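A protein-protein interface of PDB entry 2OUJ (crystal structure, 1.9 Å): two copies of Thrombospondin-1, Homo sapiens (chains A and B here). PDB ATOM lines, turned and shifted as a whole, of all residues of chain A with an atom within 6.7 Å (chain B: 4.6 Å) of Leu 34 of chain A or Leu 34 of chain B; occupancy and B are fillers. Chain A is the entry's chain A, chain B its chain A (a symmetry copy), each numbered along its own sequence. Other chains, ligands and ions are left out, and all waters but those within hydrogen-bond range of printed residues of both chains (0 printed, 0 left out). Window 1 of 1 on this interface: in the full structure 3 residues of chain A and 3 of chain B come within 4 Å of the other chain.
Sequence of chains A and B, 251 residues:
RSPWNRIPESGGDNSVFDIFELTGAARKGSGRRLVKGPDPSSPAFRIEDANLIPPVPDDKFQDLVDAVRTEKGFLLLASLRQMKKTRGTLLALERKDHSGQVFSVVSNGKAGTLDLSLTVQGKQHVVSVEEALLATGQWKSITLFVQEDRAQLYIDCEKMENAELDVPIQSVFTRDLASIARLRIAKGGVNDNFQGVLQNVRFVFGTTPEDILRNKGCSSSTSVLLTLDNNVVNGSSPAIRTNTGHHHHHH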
ATOM      1  N   ALA A  25     -19.620  19.534  10.343  1.00  0.00           N
ATOM      2  CA  ALA A  25     -19.710  20.748  11.148  1.00  0.00           C
ATOM      3  C   ALA A  25     -19.653  20.567  12.658  1.00  0.00           C
ATOM      4  O   ALA A  25     -19.149  21.436  13.368  1.00  0.00           O
ATOM      5  CB  ALA A  25     -20.974  21.506  10.775  1.00  0.00           C
ATOM      6  N   ALA A  26     -20.179  19.453  13.154  1.00  0.00           N
ATOM      7  CA  ALA A  26     -20.170  19.198  14.589  1.00  0.00           C
ATOM      8  C   ALA A  26     -18.817  18.697  15.085  1.00  0.00           C
ATOM      9  O   ALA A  26     -18.663  17.511  15.384  1.00  0.00           O
ATOM     10  CB  ALA A  26     -21.263  18.198  14.945  1.00  0.00           C
ATOM     11  N   ARG A  27     -17.831  19.592  15.166  1.00  0.00           N
ATOM     12  CA  ARG A  27     -16.517  19.181  15.653  1.00  0.00           C
ATOM     13  C   ARG A  27     -15.849  20.050  16.739  1.00  0.00           C
ATOM     14  O   ARG A  27     -15.042  20.943  16.460  1.00  0.00           O
ATOM     15  CB  ARG A  27     -15.556  18.929  14.475  1.00  0.00           C
ATOM     16  CG  ARG A  27     -14.992  20.135  13.745  1.00  0.00           C
ATOM     17  CD  ARG A  27     -13.607  19.736  13.249  1.00  0.00           C
ATOM     18  NE  ARG A  27     -12.984  20.685  12.334  1.00  0.00           N
ATOM     19  CZ  ARG A  27     -11.783  20.499  11.792  1.00  0.00           C
ATOM     20  NH1 ARG A  27     -11.091  19.403  12.083  1.00  0.00           N
ATOM     21  NH2 ARG A  27     -11.273  21.399  10.961  1.00  0.00           N
ATOM     22  N   LYS A  28     -16.220  19.725  17.979  1.00  0.00           N
ATOM     23  CA  LYS A  28     -15.778  20.314  19.255  1.00  0.00           C
ATOM     24  C   LYS A  28     -15.716  21.805  19.592  1.00  0.00           C
ATOM     25  O   LYS A  28     -15.932  22.170  20.745  1.00  0.00           O
ATOM     26  CB  LYS A  28     -14.438  19.704  19.690  1.00  0.00           C
ATOM     27  CG  LYS A  28     -14.262  19.832  21.200  1.00  0.00           C
ATOM     28  CD  LYS A  28     -12.827  19.737  21.679  1.00  0.00           C
ATOM     29  CE  LYS A  28     -12.787  19.982  23.187  1.00  0.00           C
ATOM     30  NZ  LYS A  28     -11.413  20.027  23.758  1.00  0.00           N
ATOM     31  N   ARG A  32     -17.850  27.378  15.581  1.00  0.00           N
ATOM     32  CA  ARG A  32     -19.224  27.548  16.042  1.00  0.00           C
ATOM     33  C   ARG A  32     -19.566  26.878  17.369  1.00  0.00           C
ATOM     34  O   ARG A  32     -18.908  25.930  17.799  1.00  0.00           O
ATOM     35  CB  ARG A  32     -20.206  27.095  14.953  1.00  0.00           C
ATOM     36  CG  ARG A  32     -19.828  25.818  14.210  1.00  0.00           C
ATOM     37  CD  ARG A  32     -19.883  24.588  15.094  1.00  0.00           C
ATOM     38  NE  ARG A  32     -18.565  24.178  15.569  1.00  0.00           N
ATOM     39  CZ  ARG A  32     -18.343  23.083  16.291  1.00  0.00           C
ATOM     40  NH1 ARG A  32     -19.354  22.289  16.624  1.00  0.00           N
ATOM     41  NH2 ARG A  32     -17.111  22.774  16.667  1.00  0.00           N
ATOM     42  N   ARG A  33     -20.611  27.394  18.008  1.00  0.00           N
ATOM     43  CA  ARG A  33     -21.081  26.893  19.294  1.00  0.00           C
ATOM     44  C   ARG A  33     -22.430  26.196  19.097  1.00  0.00           C
ATOM     45  O   ARG A  33     -23.377  26.793  18.582  1.00  0.00           O
ATOM     46  CB  ARG A  33     -21.245  28.064  20.273  1.00  0.00           C
ATOM     47  CG  ARG A  33     -20.969  27.740  21.736  1.00  0.00           C
ATOM     48  CD  ARG A  33     -19.560  28.171  22.136  1.00  0.00           C
ATOM     49  NE  ARG A  33     -19.271  27.892  23.543  1.00  0.00           N
ATOM     50  CZ  ARG A  33     -18.056  27.955  24.084  1.00  0.00           C
ATOM     51  NH1 ARG A  33     -17.010  28.291  23.338  1.00  0.00           N
ATOM     52  NH2 ARG A  33     -17.886  27.678  25.369  1.00  0.00           N
ATOM     53  N   LEU A  34     -22.510  24.934  19.505  1.00  0.00           N
ATOM     54  CA  LEU A  34     -23.737  24.154  19.375  1.00  0.00           C
ATOM     55  C   LEU A  34     -24.820  24.744  20.275  1.00  0.00           C
ATOM     56  O   LEU A  34     -24.650  24.818  21.490  1.00  0.00           O
ATOM     57  CB  LEU A  34     -23.460  22.703  19.768  1.00  0.00           C
ATOM     58  CG  LEU A  34     -22.219  22.115  19.082  1.00  0.00           C
ATOM     59  CD1 LEU A  34     -21.772  20.854  19.799  1.00  0.00           C
ATOM     60  CD2 LEU A  34     -22.518  21.842  17.616  1.00  0.00           C
ATOM     61  N   VAL A  35     -25.932  25.168  19.680  1.00  0.00           N
ATOM     62  CA  VAL A  35     -27.017  25.757  20.454  1.00  0.00           C
ATOM     63  C   VAL A  35     -28.410  25.244  20.092  1.00  0.00           C
ATOM     64  O   VAL A  35     -28.559  24.258  19.368  1.00  0.00           O
ATOM     65  CB  VAL A  35     -27.016  27.300  20.329  1.00  0.00           C
ATOM     66  CG1 VAL A  35     -25.688  27.861  20.809  1.00  0.00           C
ATOM     67  CG2 VAL A  35     -27.277  27.707  18.885  1.00  0.00           C
ATOM     68  N   LYS A  36     -29.423  25.938  20.607  1.00  0.00           N
ATOM     69  CA  LYS A  36     -30.827  25.593  20.400  1.00  0.00           C
ATOM     70  C   LYS A  36     -31.403  26.116  19.084  1.00  0.00           C
ATOM     71  O   LYS A  36     -31.074  27.218  18.644  1.00  0.00           O
ATOM     72  CB  LYS A  36     -31.653  26.147  21.565  1.00  0.00           C
ATOM     73  CG  LYS A  36     -33.121  25.760  21.562  1.00  0.00           C
ATOM     74  CD  LYS A  36     -33.910  26.656  22.507  1.00  0.00           C
ATOM     75  CE  LYS A  36     -35.283  26.073  22.824  1.00  0.00           C
ATOM     76  NZ  LYS A  36     -36.062  25.715  21.604  1.00  0.00           N
ATOM     77  N   PRO A  43     -29.360  19.886  15.661  1.00  0.00           N
ATOM     78  CA  PRO A  43     -28.459  20.870  16.271  1.00  0.00           C
ATOM     79  C   PRO A  43     -28.385  22.187  15.498  1.00  0.00           C
ATOM     80  O   PRO A  43     -28.392  22.197  14.267  1.00  0.00           O
ATOM     81  CB  PRO A  43     -27.121  20.136  16.285  1.00  0.00           C
ATOM     82  CG  PRO A  43     -27.178  19.353  15.014  1.00  0.00           C
ATOM     83  CD  PRO A  43     -28.591  18.796  15.031  1.00  0.00           C
ATOM     84  N   ALA A  44     -28.336  23.292  16.236  1.00  0.00           N
ATOM     85  CA  ALA A  44     -28.238  24.623  15.647  1.00  0.00           C
ATOM     86  C   ALA A  44     -26.841  25.161  15.953  1.00  0.00           C
ATOM     87  O   ALA A  44     -26.319  24.950  17.047  1.00  0.00           O
ATOM     88  CB  ALA A  44     -29.302  25.541  16.236  1.00  0.00           C
ATOM     89  N   PHE A  45     -26.239  25.855  14.991  1.00  0.00           N
ATOM     90  CA  PHE A  45     -24.890  26.390  15.167  1.00  0.00           C
ATOM     91  C   PHE A  45     -24.830  27.910  15.220  1.00  0.00           C
ATOM     92  O   PHE A  45     -25.274  28.582  14.286  1.00  0.00           O
ATOM     93  CB  PHE A  45     -23.968  25.944  14.021  1.00  0.00           C
ATOM     94  CG  PHE A  45     -23.960  24.463  13.766  1.00  0.00           C
ATOM     95  CD1 PHE A  45     -25.109  23.801  13.350  1.00  0.00           C
ATOM     96  CD2 PHE A  45     -22.783  23.736  13.899  1.00  0.00           C
ATOM     97  CE1 PHE A  45     -25.087  22.442  13.066  1.00  0.00           C
ATOM     98  CE2 PHE A  45     -22.748  22.372  13.616  1.00  0.00           C
ATOM     99  CZ  PHE A  45     -23.901  21.724  13.200  1.00  0.00           C
ATOM    100  N   ARG A  46     -24.293  28.456  16.306  1.00  0.00           N
ATOM    101  CA  ARG A  46     -24.137  29.901  16.395  1.00  0.00           C
ATOM    102  C   ARG A  46     -22.727  30.108  15.852  1.00  0.00           C
ATOM    103  O   ARG A  46     -21.758  29.578  16.404  1.00  0.00           O
ATOM    104  CB  ARG A  46     -24.253  30.395  17.844  1.00  0.00           C
ATOM    105  CG  ARG A  46     -24.184  31.921  17.975  1.00  0.00           C
ATOM    106  CD  ARG A  46     -24.964  32.432  19.185  1.00  0.00           C
ATOM    107  NE  ARG A  46     -26.160  33.183  18.798  1.00  0.00           N
ATOM    108  CZ  ARG A  46     -26.149  34.404  18.266  1.00  0.00           C
ATOM    109  NH1 ARG A  46     -24.998  35.031  18.053  1.00  0.00           N
ATOM    110  NH2 ARG A  46     -27.290  35.001  17.940  1.00  0.00           N
ATOM    111  N   GLU A  48     -19.109  31.541  14.949  1.00  0.00           N
ATOM    112  CA  GLU A  48     -18.066  32.245  15.685  1.00  0.00           C
ATOM    113  C   GLU A  48     -16.907  32.578  14.752  1.00  0.00           C
ATOM    114  O   GLU A  48     -16.356  33.681  14.792  1.00  0.00           O
ATOM    115  CB  GLU A  48     -17.572  31.381  16.850  1.00  0.00           C
ATOM    116  CG  GLU A  48     -18.606  31.186  17.950  1.00  0.00           C
ATOM    117  CD  GLU A  48     -18.149  30.221  19.033  1.00  0.00           C
ATOM    118  OE1 GLU A  48     -18.724  30.259  20.146  1.00  0.00           O
ATOM    119  OE2 GLU A  48     -17.225  29.417  18.771  1.00  0.00           O
ATOM    120  N   ARG B  32     -25.399  24.140  31.457  1.00  0.00           N
ATOM    121  CA  ARG B  32     -24.521  23.320  30.628  1.00  0.00           C
ATOM    122  C   ARG B  32     -24.323  23.804  29.194  1.00  0.00           C
ATOM    123  O   ARG B  32     -25.142  24.541  28.645  1.00  0.00           O
ATOM    124  CB  ARG B  32     -25.001  21.862  30.632  1.00  0.00           C
ATOM    125  CG  ARG B  32     -26.510  21.662  30.535  1.00  0.00           C
ATOM    126  CD  ARG B  32     -27.073  22.084  29.193  1.00  0.00           C
ATOM    127  NE  ARG B  32     -27.695  23.404  29.234  1.00  0.00           N
ATOM    128  CZ  ARG B  32     -28.330  23.959  28.206  1.00  0.00           C
ATOM    129  NH1 ARG B  32     -28.424  23.308  27.052  1.00  0.00           N
ATOM    130  NH2 ARG B  32     -28.882  25.156  28.334  1.00  0.00           N
ATOM    131  N   ARG B  33     -23.214  23.370  28.603  1.00  0.00           N
ATOM    132  CA  ARG B  33     -22.849  23.735  27.239  1.00  0.00           C
ATOM    133  C   ARG B  33     -22.976  22.501  26.340  1.00  0.00           C
ATOM    134  O   ARG B  33     -22.366  21.464  26.605  1.00  0.00           O
ATOM    135  CB  ARG B  33     -21.401  24.243  27.213  1.00  0.00           C
ATOM    136  CG  ARG B  33     -21.101  25.319  26.177  1.00  0.00           C
ATOM    137  CD  ARG B  33     -21.116  26.708  26.810  1.00  0.00           C
ATOM    138  NE  ARG B  33     -20.812  27.764  25.845  1.00  0.00           N
ATOM    139  CZ  ARG B  33     -20.984  29.063  26.077  1.00  0.00           C
ATOM    140  NH1 ARG B  33     -21.459  29.475  27.248  1.00  0.00           N
ATOM    141  NH2 ARG B  33     -20.687  29.952  25.139  1.00  0.00           N
ATOM    142  N   LEU B  34     -23.772  22.620  25.283  1.00  0.00           N
ATOM    143  CA  LEU B  34     -23.983  21.520  24.345  1.00  0.00           C
ATOM    144  C   LEU B  34     -22.681  21.216  23.608  1.00  0.00           C
ATOM    145  O   LEU B  34     -22.134  22.079  22.924  1.00  0.00           O
ATOM    146  CB  LEU B  34     -25.075  21.906  23.348  1.00  0.00           C
ATOM    147  CG  LEU B  34     -26.338  22.464  24.017  1.00  0.00           C
ATOM    148  CD1 LEU B  34     -27.195  23.189  22.995  1.00  0.00           C
ATOM    149  CD2 LEU B  34     -27.109  21.339  24.689  1.00  0.00           C
ATOM    150  N   VAL B  35     -22.183  19.990  23.747  1.00  0.00           N
ATOM    151  CA  VAL B  35     -20.938  19.609  23.091  1.00  0.00           C
ATOM    152  C   VAL B  35     -20.977  18.251  22.392  1.00  0.00           C
ATOM    153  O   VAL B  35     -22.039  17.653  22.216  1.00  0.00           O
ATOM    154  CB  VAL B  35     -19.758  19.610  24.093  1.00  0.00           C
ATOM    155  CG1 VAL B  35     -19.603  20.988  24.714  1.00  0.00           C
ATOM    156  CG2 VAL B  35     -19.988  18.561  25.173  1.00  0.00           C
ATOM    157  N   LYS B  36     -19.794  17.779  22.002  1.00  0.00           N
ATOM    158  CA  LYS B  36     -19.623  16.513  21.294  1.00  0.00           C
ATOM    159  C   LYS B  36     -19.580  15.293  22.215  1.00  0.00           C
ATOM    160  O   LYS B  36     -19.024  15.348  23.312  1.00  0.00           O
ATOM    161  CB  LYS B  36     -18.328  16.570  20.476  1.00  0.00           C
ATOM    162  CG  LYS B  36     -18.073  15.372  19.580  1.00  0.00           C
ATOM    163  CD  LYS B  36     -16.619  15.346  19.129  1.00  0.00           C
ATOM    164  CE  LYS B  36     -16.412  14.405  17.946  1.00  0.00           C
ATOM    165  NZ  LYS B  36     -16.954  13.036  18.186  1.00  0.00           N
ATOM    166  N   ALA B  44     -24.326  15.921  23.816  1.00  0.00           N
ATOM    167  CA  ALA B  44     -23.565  15.714  25.043  1.00  0.00           C
ATOM    168  C   ALA B  44     -23.534  17.042  25.796  1.00  0.00           C
ATOM    169  O   ALA B  44     -23.407  18.102  25.184  1.00  0.00           O
ATOM    170  CB  ALA B  44     -22.149  15.255  24.715  1.00  0.00           C
ATOM    171  N   PHE B  45     -23.648  16.986  27.121  1.00  0.00           N
ATOM    172  CA  PHE B  45     -23.660  18.198  27.937  1.00  0.00           C
ATOM    173  C   PHE B  45     -22.440  18.351  28.834  1.00  0.00           C
ATOM    174  O   PHE B  45     -22.155  17.472  29.650  1.00  0.00           O
ATOM    175  CB  PHE B  45     -24.895  18.234  28.850  1.00  0.00           C
ATOM    176  CG  PHE B  45     -26.204  18.018  28.141  1.00  0.00           C
ATOM    177  CD1 PHE B  45     -26.480  16.816  27.499  1.00  0.00           C
ATOM    178  CD2 PHE B  45     -27.181  19.005  28.156  1.00  0.00           C
ATOM    179  CE1 PHE B  45     -27.707  16.599  26.888  1.00  0.00           C
ATOM    180  CE2 PHE B  45     -28.417  18.799  27.547  1.00  0.00           C
ATOM    181  CZ  PHE B  45     -28.680  17.595  26.912  1.00  0.00           C
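Among the printed residues, merely in contact across the chains: Leu 34 of chain A with Leu 34 of chain B, Leu 34 of chain A with Val 35 of chain B and Val 35 of chain A with Leu 34 of chain B.
Printed residues of chain B that touch a printed residue of chain A: Arg 33, Leu 34 and Val 35.
Hydrophobic or aromatic side chains of chain B within 4 Å of the printed part of chain A: Leu 34.
Of the 14 printed residues of chain A, 3 touch a printed residue of chain B.
Among the printed residues, 4 pairs touch across the chains.
Of chain B, only Leu 34 and Val 35 come within 4 Å of Leu 34 of chain A.
Leu 34 of chain B touches just these residues of chain A: Leu 34 and Val 35.
Of the printed residues of chain B, Arg 33 of chain A touches Arg 33 (2.8 Å).
Of the printed residues of chain A, Val 35 of chain B touches Leu 34 (3.6 Å).
Printed residues of chain A within 4 Å of Arg 33 of chain B: Arg 33 (2.8 Å).
Printed residues of chain B within 4 Å of Val 35 of chain A: Leu 34.
Phe 45 of chain A touches none of the printed residues of chain B.
Arg 33 of chain A touches its own counterpart, Arg 33 of chain B.
Leu 34 of chain B touches its own counterpart, Leu 34 of chain A.
Leu 34 of chain A touches Val 35 of chain B, and with the chains exchanged Val 35 of chain A touches Leu 34 of chain B.
N of Arg 33 of chain A lies within hydrogen-bond range of O of Arg 46 of chain A, 2.9 Å away.
The backbone carbonyl oxygen (O) of Ala 44 of chain B sits at hydrogen-bond distance from the backbone NH (N) of Val 35 of chain B (2.7 Å).
The backbone NH of Val 35 of chain A lies within hydrogen-bond range of the backbone carbonyl oxygen of Ala 44 of chain A, at 2.7 Å.
The guanidinium group (NE) of Arg 33 of chain A sits close to the guanidinium group (NE) of Arg 33 of chain B (2.8 Å).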
